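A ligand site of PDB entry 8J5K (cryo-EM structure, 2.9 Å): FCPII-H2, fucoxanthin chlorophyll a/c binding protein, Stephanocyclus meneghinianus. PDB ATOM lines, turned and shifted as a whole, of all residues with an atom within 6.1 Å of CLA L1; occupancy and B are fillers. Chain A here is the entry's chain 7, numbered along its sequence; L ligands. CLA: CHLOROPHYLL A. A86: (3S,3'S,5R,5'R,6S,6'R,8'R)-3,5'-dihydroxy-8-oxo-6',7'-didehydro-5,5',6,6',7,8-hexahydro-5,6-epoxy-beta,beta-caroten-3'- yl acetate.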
ATOM      1  N   ILE A   8      -2.098  23.856  -0.912  1.00  0.00           N
ATOM      2  CA  ILE A   8      -2.464  22.482  -1.256  1.00  0.00           C
ATOM      3  C   ILE A   8      -3.994  22.420  -1.333  1.00  0.00           C
ATOM      4  O   ILE A   8      -4.659  23.440  -1.124  1.00  0.00           O
ATOM      5  CB  ILE A   8      -1.846  21.478  -0.252  1.00  0.00           C
ATOM      6  CG1 ILE A   8      -0.323  21.554  -0.341  1.00  0.00           C
ATOM      7  CG2 ILE A   8      -2.203  20.042  -0.549  1.00  0.00           C
ATOM      8  CD1 ILE A   8       0.386  20.819   0.745  1.00  0.00           C
ATOM      9  N   ALA A   9      -4.561  21.264  -1.700  1.00  0.00           N
ATOM     10  CA  ALA A   9      -5.990  21.177  -1.973  1.00  0.00           C
ATOM     11  C   ALA A   9      -6.866  21.429  -0.745  1.00  0.00           C
ATOM     12  O   ALA A   9      -7.746  22.293  -0.815  1.00  0.00           O
ATOM     13  CB  ALA A   9      -6.320  19.838  -2.627  1.00  0.00           C
ATOM     14  N   PRO A  10      -6.702  20.722   0.383  1.00  0.00           N
ATOM     15  CA  PRO A  10      -7.565  21.030   1.529  1.00  0.00           C
ATOM     16  C   PRO A  10      -7.247  22.430   2.019  1.00  0.00           C
ATOM     17  O   PRO A  10      -6.127  22.645   2.504  1.00  0.00           O
ATOM     18  CB  PRO A  10      -7.201  19.960   2.553  1.00  0.00           C
ATOM     19  CG  PRO A  10      -5.776  19.662   2.265  1.00  0.00           C
ATOM     20  CD  PRO A  10      -5.643  19.767   0.762  1.00  0.00           C
ATOM     21  N   GLU A 117       8.511  20.542  -4.813  1.00  0.00           N
ATOM     22  CA  GLU A 117       7.568  19.560  -4.329  1.00  0.00           C
ATOM     23  C   GLU A 117       8.047  19.037  -3.007  1.00  0.00           C
ATOM     24  O   GLU A 117       7.251  18.732  -2.136  1.00  0.00           O
ATOM     25  CB  GLU A 117       7.450  18.428  -5.322  1.00  0.00           C
ATOM     26  CG  GLU A 117       7.048  17.093  -4.715  1.00  0.00           C
ATOM     27  CD  GLU A 117       5.782  16.552  -5.334  1.00  0.00           C
ATOM     28  OE1 GLU A 117       4.927  17.368  -5.726  1.00  0.00           O
ATOM     29  OE2 GLU A 117       5.641  15.320  -5.417  1.00  0.00           O
ATOM     30  N   LEU A 120       7.401  21.836  -0.351  1.00  0.00           N
ATOM     31  CA  LEU A 120       6.016  21.827   0.083  1.00  0.00           C
ATOM     32  C   LEU A 120       5.748  20.693   1.063  1.00  0.00           C
ATOM     33  O   LEU A 120       5.008  20.863   2.045  1.00  0.00           O
ATOM     34  CB  LEU A 120       5.092  21.730  -1.128  1.00  0.00           C
ATOM     35  CG  LEU A 120       3.616  21.997  -0.899  1.00  0.00           C
ATOM     36  CD1 LEU A 120       3.421  23.263  -0.106  1.00  0.00           C
ATOM     37  CD2 LEU A 120       2.908  22.091  -2.238  1.00  0.00           C
ATOM     38  N   GLN A 121       6.324  19.516   0.800  1.00  0.00           N
ATOM     39  CA  GLN A 121       6.183  18.404   1.740  1.00  0.00           C
ATOM     40  C   GLN A 121       6.770  18.772   3.101  1.00  0.00           C
ATOM     41  O   GLN A 121       6.176  18.476   4.144  1.00  0.00           O
ATOM     42  CB  GLN A 121       6.870  17.160   1.190  1.00  0.00           C
ATOM     43  CG  GLN A 121       6.200  16.546  -0.030  1.00  0.00           C
ATOM     44  CD  GLN A 121       7.095  15.560  -0.742  1.00  0.00           C
ATOM     45  OE1 GLN A 121       8.281  15.436  -0.424  1.00  0.00           O
ATOM     46  NE2 GLN A 121       6.535  14.837  -1.708  1.00  0.00           N
ATOM     47  N   GLU A 122       7.939  19.413   3.093  1.00  0.00           N
ATOM     48  CA  GLU A 122       8.552  19.843   4.341  1.00  0.00           C
ATOM     49  C   GLU A 122       7.652  20.814   5.101  1.00  0.00           C
ATOM     50  O   GLU A 122       7.430  20.664   6.313  1.00  0.00           O
ATOM     51  CB  GLU A 122       9.902  20.490   4.050  1.00  0.00           C
ATOM     52  CG  GLU A 122      10.670  20.932   5.270  1.00  0.00           C
ATOM     53  CD  GLU A 122      12.039  21.463   4.917  1.00  0.00           C
ATOM     54  OE1 GLU A 122      12.334  21.634   3.716  1.00  0.00           O
ATOM     55  OE2 GLU A 122      12.832  21.723   5.843  1.00  0.00           O
ATOM     56  N   GLN A 124       4.353  21.214   4.882  1.00  0.00           N
ATOM     57  CA  GLN A 124       3.134  20.585   5.363  1.00  0.00           C
ATOM     58  C   GLN A 124       3.408  19.679   6.558  1.00  0.00           C
ATOM     59  O   GLN A 124       2.621  19.636   7.518  1.00  0.00           O
ATOM     60  CB  GLN A 124       2.457  19.814   4.238  1.00  0.00           C
ATOM     61  CG  GLN A 124       0.977  19.598   4.463  1.00  0.00           C
ATOM     62  CD  GLN A 124       0.134  20.777   4.020  1.00  0.00           C
ATOM     63  OE1 GLN A 124       0.568  21.931   4.090  1.00  0.00           O
ATOM     64  NE2 GLN A 124      -1.066  20.499   3.557  1.00  0.00           N
ATOM     65  N   HIS A 125       4.515  18.940   6.510  1.00  0.00           N
ATOM     66  CA  HIS A 125       4.907  18.139   7.664  1.00  0.00           C
ATOM     67  C   HIS A 125       5.130  19.033   8.874  1.00  0.00           C
ATOM     68  O   HIS A 125       4.753  18.660   9.997  1.00  0.00           O
ATOM     69  CB  HIS A 125       6.166  17.345   7.342  1.00  0.00           C
ATOM     70  CG  HIS A 125       5.918  16.101   6.568  1.00  0.00           C
ATOM     71  ND1 HIS A 125       5.226  16.094   5.382  1.00  0.00           N
ATOM     72  CD2 HIS A 125       6.264  14.818   6.813  1.00  0.00           C
ATOM     73  CE1 HIS A 125       5.162  14.863   4.918  1.00  0.00           C
ATOM     74  NE2 HIS A 125       5.787  14.066   5.762  1.00  0.00           N
ATOM     75  N   LEU A 128       1.751  20.046  10.369  1.00  0.00           N
ATOM     76  CA  LEU A 128       1.160  18.990  11.185  1.00  0.00           C
ATOM     77  C   LEU A 128       1.917  18.801  12.501  1.00  0.00           C
ATOM     78  O   LEU A 128       1.306  18.611  13.566  1.00  0.00           O
ATOM     79  CB  LEU A 128       1.106  17.685  10.404  1.00  0.00           C
ATOM     80  CG  LEU A 128       0.635  16.469  11.218  1.00  0.00           C
ATOM     81  CD1 LEU A 128      -0.792  16.685  11.690  1.00  0.00           C
ATOM     82  CD2 LEU A 128       0.751  15.202  10.401  1.00  0.00           C
HETATM   83 MG   CLA L   1      -2.703  16.320   2.636  1.00  0.00          MG
HETATM   84  CHA CLA L   1       0.461  16.067   1.223  1.00  0.00           C
HETATM   85  CHB CLA L   1      -4.084  16.256  -0.478  1.00  0.00           C
HETATM   86  CHC CLA L   1      -5.814  16.446   4.078  1.00  0.00           C
HETATM   87  CHD CLA L   1      -1.228  16.226   5.848  1.00  0.00           C
HETATM   88  NA  CLA L   1      -1.912  16.213   0.704  1.00  0.00           N
HETATM   89  C1A CLA L   1      -0.566  16.107   0.316  1.00  0.00           C
HETATM   90  C2A CLA L   1      -0.445  16.038  -1.204  1.00  0.00           C
HETATM   91  C3A CLA L   1      -1.896  16.130  -1.704  1.00  0.00           C
HETATM   92  C4A CLA L   1      -2.708  16.211  -0.412  1.00  0.00           C
HETATM   93  CMA CLA L   1      -2.134  17.275  -2.657  1.00  0.00           C
HETATM   94  CAA CLA L   1       0.141  14.702  -1.635  1.00  0.00           C
HETATM   95  NB  CLA L   1      -4.594  16.349   1.936  1.00  0.00           N
HETATM   96  C1B CLA L   1      -4.957  16.319   0.633  1.00  0.00           C
HETATM   97  C2B CLA L   1      -6.434  16.334   0.514  1.00  0.00           C
HETATM   98  C3B CLA L   1      -6.936  16.389   1.800  1.00  0.00           C
HETATM   99  C4B CLA L   1      -5.772  16.398   2.719  1.00  0.00           C
HETATM  100  CMB CLA L   1      -7.144  16.298  -0.759  1.00  0.00           C
HETATM  101  CAB CLA L   1      -8.304  16.431   2.242  1.00  0.00           C
HETATM  102  CBB CLA L   1      -8.868  15.604   3.120  1.00  0.00           C
HETATM  103  NC  CLA L   1      -3.381  16.374   4.600  1.00  0.00           N
HETATM  104  C1C CLA L   1      -4.701  16.441   4.971  1.00  0.00           C
HETATM  105  C2C CLA L   1      -4.824  16.460   6.417  1.00  0.00           C
HETATM  106  C3C CLA L   1      -3.524  16.370   6.919  1.00  0.00           C
HETATM  107  C4C CLA L   1      -2.628  16.310   5.778  1.00  0.00           C
HETATM  108  CMC CLA L   1      -6.084  16.545   7.151  1.00  0.00           C
HETATM  109  CAC CLA L   1      -3.125  16.344   8.334  1.00  0.00           C
HETATM  110  CBC CLA L   1      -2.704  14.963   8.777  1.00  0.00           C
HETATM  111  ND  CLA L   1      -0.850  16.268   3.422  1.00  0.00           N
HETATM  112  C1D CLA L   1      -0.382  16.197   4.763  1.00  0.00           C
HETATM  113  C2D CLA L   1       1.094  16.116   4.754  1.00  0.00           C
HETATM  114  C3D CLA L   1       1.461  16.086   3.428  1.00  0.00           C
HETATM  115  C4D CLA L   1       0.228  16.151   2.633  1.00  0.00           C
HETATM  116  CMD CLA L   1       1.920  16.077   5.956  1.00  0.00           C
HETATM  117  CAD CLA L   1       2.566  16.028   2.490  1.00  0.00           C
HETATM  118  OBD CLA L   1       3.781  16.061   2.691  1.00  0.00           O
HETATM  119  CBD CLA L   1       1.959  15.928   1.069  1.00  0.00           C
HETATM  120  CGD CLA L   1       2.592  16.968   0.192  1.00  0.00           C
HETATM  121  O1D CLA L   1       3.237  17.956   0.557  1.00  0.00           O
HETATM  122  O2D CLA L   1       2.452  16.775  -1.147  1.00  0.00           O
HETATM  123  CED CLA L   1       2.649  17.893  -2.007  1.00  0.00           C
HETATM  124  C   A86 L   2     -10.788  24.616  19.726  1.00  0.00           C
HETATM  125  O   A86 L   2      -5.387  18.894   9.516  1.00  0.00           O
HETATM  126  C1  A86 L   2     -10.408  23.365  20.456  1.00  0.00           C
HETATM  127  C10 A86 L   2      -5.979  20.473  12.377  1.00  0.00           C
HETATM  128  C11 A86 L   2      -5.314  19.528  11.713  1.00  0.00           C
HETATM  129  C12 A86 L   2      -4.915  18.254  12.398  1.00  0.00           C
HETATM  130  C13 A86 L   2      -4.984  19.719  10.309  1.00  0.00           C
HETATM  131  C14 A86 L   2      -4.101  20.853   9.831  1.00  0.00           C
HETATM  132  C15 A86 L   2      -3.964  20.901   8.308  1.00  0.00           C
HETATM  133  C16 A86 L   2      -5.150  21.567   7.566  1.00  0.00           C
HETATM  134  C17 A86 L   2      -5.100  21.567   6.040  1.00  0.00           C
HETATM  135  C18 A86 L   2      -3.820  22.238   5.637  1.00  0.00           C
HETATM  136  C19 A86 L   2      -2.653  21.369   6.090  1.00  0.00           C
HETATM  137  C2  A86 L   2      -9.655  22.432  19.857  1.00  0.00           C
HETATM  138  C20 A86 L   2      -2.653  20.870   7.531  1.00  0.00           C
HETATM  139  C21 A86 L   2      -1.395  20.115   7.910  1.00  0.00           C
HETATM  140  C22 A86 L   2      -5.124  23.029   8.016  1.00  0.00           C
HETATM  141  C23 A86 L   2      -6.544  21.063   7.897  1.00  0.00           C
HETATM  142  C24 A86 L   2     -10.863  23.142  21.836  1.00  0.00           C
HETATM  143  C25 A86 L   2     -11.636  24.013  22.466  1.00  0.00           C
HETATM  144  C26 A86 L   2     -12.025  23.669  23.823  1.00  0.00           C
HETATM  145  C27 A86 L   2     -12.813  24.430  24.608  1.00  0.00           C
HETATM  146  C28 A86 L   2     -13.375  25.740  24.151  1.00  0.00           C
HETATM  147  C29 A86 L   2     -13.086  23.887  25.951  1.00  0.00           C
HETATM  148  C3  A86 L   2      -9.215  22.629  18.484  1.00  0.00           C
HETATM  149  C30 A86 L   2     -13.769  24.377  26.889  1.00  0.00           C
HETATM  150  C31 A86 L   2     -14.399  24.706  27.917  1.00  0.00           C
HETATM  151  C32 A86 L   2     -15.783  25.329  27.792  1.00  0.00           C
HETATM  152  C33 A86 L   2     -16.576  25.024  29.068  1.00  0.00           C
HETATM  153  C34 A86 L   2     -15.895  25.589  30.332  1.00  0.00           C
HETATM  154  C35 A86 L   2     -14.619  24.775  30.324  1.00  0.00           C
HETATM  155  C36 A86 L   2     -13.607  24.895  29.172  1.00  0.00           C
HETATM  156  C37 A86 L   2     -12.817  26.203  29.216  1.00  0.00           C
HETATM  157  C38 A86 L   2     -16.890  27.807  30.481  1.00  0.00           C
HETATM  158  C39 A86 L   2     -17.054  28.680  31.694  1.00  0.00           C
HETATM  159  C4  A86 L   2      -8.491  21.696  17.870  1.00  0.00           C
HETATM  160  C40 A86 L   2     -15.641  26.811  27.438  1.00  0.00           C
HETATM  161  C41 A86 L   2     -16.487  24.640  26.629  1.00  0.00           C
HETATM  162  C5  A86 L   2      -8.079  21.903  16.486  1.00  0.00           C
HETATM  163  C6  A86 L   2      -7.375  20.964  15.844  1.00  0.00           C
HETATM  164  C7  A86 L   2      -6.985  19.696  16.542  1.00  0.00           C
HETATM  165  C8  A86 L   2      -6.999  21.186  14.440  1.00  0.00           C
HETATM  166  C9  A86 L   2      -6.324  20.248  13.782  1.00  0.00           C
HETATM  167  O1  A86 L   2      -2.910  21.892   8.456  1.00  0.00           O
HETATM  168  O2  A86 L   2      -3.782  22.351   4.217  1.00  0.00           O
HETATM  169  O3  A86 L   2     -12.678  23.810  29.275  1.00  0.00           O
HETATM  170  O4  A86 L   2     -15.677  27.007  30.380  1.00  0.00           O
HETATM  171  O5  A86 L   2     -17.750  27.760  29.618  1.00  0.00           O
HETATM  172 MG   CLA L   3       5.017  11.371   5.939  1.00  0.00          MG
HETATM  173  CHA CLA L   3       5.061  11.815   2.502  1.00  0.00           C
HETATM  174  CHB CLA L   3       8.392  10.969   5.926  1.00  0.00           C
HETATM  175  CHC CLA L   3       4.944  11.076   9.363  1.00  0.00           C
HETATM  176  CHD CLA L   3       1.521  11.908   5.918  1.00  0.00           C
HETATM  177  NA  CLA L   3       6.460  11.363   4.431  1.00  0.00           N
HETATM  178  C1A CLA L   3       6.286  11.574   3.059  1.00  0.00           C
HETATM  179  C2A CLA L   3       7.618  11.489   2.312  1.00  0.00           C
HETATM  180  C3A CLA L   3       8.639  11.127   3.420  1.00  0.00           C
HETATM  181  C4A CLA L   3       7.789  11.142   4.692  1.00  0.00           C
HETATM  182  CMA CLA L   3       9.283   9.791   3.181  1.00  0.00           C
HETATM  183  CAA CLA L   3       8.001  12.807   1.659  1.00  0.00           C
HETATM  184  CBA CLA L   3       9.248  12.652   0.826  1.00  0.00           C
HETATM  185  CGA CLA L   3       8.893  12.393  -0.603  1.00  0.00           C
HETATM  186  NB  CLA L   3       6.396  11.044   7.370  1.00  0.00           N
HETATM  187  C1B CLA L   3       7.734  10.965   7.158  1.00  0.00           C
HETATM  188  C2B CLA L   3       8.443  10.864   8.470  1.00  0.00           C
HETATM  189  C3B CLA L   3       7.473  10.897   9.447  1.00  0.00           C
HETATM  190  C4B CLA L   3       6.157  11.004   8.756  1.00  0.00           C
HETATM  191  CMB CLA L   3       9.901  10.767   8.552  1.00  0.00           C
HETATM  192  CAB CLA L   3       7.563  10.843  10.883  1.00  0.00           C
HETATM  193  CBB CLA L   3       8.581  10.345  11.603  1.00  0.00           C
HETATM  194  NC  CLA L   3       3.497  11.443   7.368  1.00  0.00           N
HETATM  195  C1C CLA L   3       3.689  11.272   8.707  1.00  0.00           C
HETATM  196  C2C CLA L   3       2.412  11.366   9.409  1.00  0.00           C
HETATM  197  C3C CLA L   3       1.449  11.631   8.441  1.00  0.00           C
HETATM  198  C4C CLA L   3       2.137  11.683   7.160  1.00  0.00           C
HETATM  199  CMC CLA L   3       2.236  11.220  10.849  1.00  0.00           C
HETATM  200  CAC CLA L   3       0.004  11.814   8.650  1.00  0.00           C
HETATM  201  CBC CLA L   3      -0.806  10.625   8.220  1.00  0.00           C
HETATM  202  ND  CLA L   3       3.576  11.720   4.581  1.00  0.00           N
HETATM  203  C1D CLA L   3       2.170  11.925   4.705  1.00  0.00           C
HETATM  204  C2D CLA L   3       1.603  12.159   3.359  1.00  0.00           C
HETATM  205  C3D CLA L   3       2.666  12.117   2.482  1.00  0.00           C
HETATM  206  C4D CLA L   3       3.872  11.860   3.294  1.00  0.00           C
HETATM  207  CMD CLA L   3       0.183  12.378   3.096  1.00  0.00           C
HETATM  208  CAD CLA L   3       3.083  12.210   1.094  1.00  0.00           C
HETATM  209  OBD CLA L   3       2.403  12.369   0.083  1.00  0.00           O
HETATM  210  CBD CLA L   3       4.633  12.062   1.069  1.00  0.00           C
HETATM  211  CGD CLA L   3       5.091  10.968   0.154  1.00  0.00           C
HETATM  212  O1D CLA L   3       6.212  10.797  -0.325  1.00  0.00           O
HETATM  213  O2D CLA L   3       4.119  10.060  -0.154  1.00  0.00           O
HETATM  214  CED CLA L   3       4.479   8.685  -0.154  1.00  0.00           C
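An oxygen (OBD) of CLA L1 sits close to a ring nitrogen (ND1) of His 125, 3.1 Å away.
An oxygen (O1D) of CLA L1 lies close to the backbone NH (N) of Gln 121 (3.5 Å).
O of Pro 10 lies within hydrogen-bond range of O2 of A86 L2 (2.9 Å).
The side-chain amide nitrogen (NE2) of Gln 124 lies close to an oxygen (O2) of A86 L2.
O of Gln 121 lies within hydrogen-bond range of ND1 of His 125 (2.8 Å).
Residues that only touch CLA L1: Ile 8, Pro 10, Leu 120, Gln 124 and Leu 128.
Hydrophobic or aromatic side chains within 4 Å of CLA L1: Ile 8, Pro 10, His 125 and Leu 128.
The nearest printed residue that does not touch CLA L1 is Ala 9 (4.1 Å).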
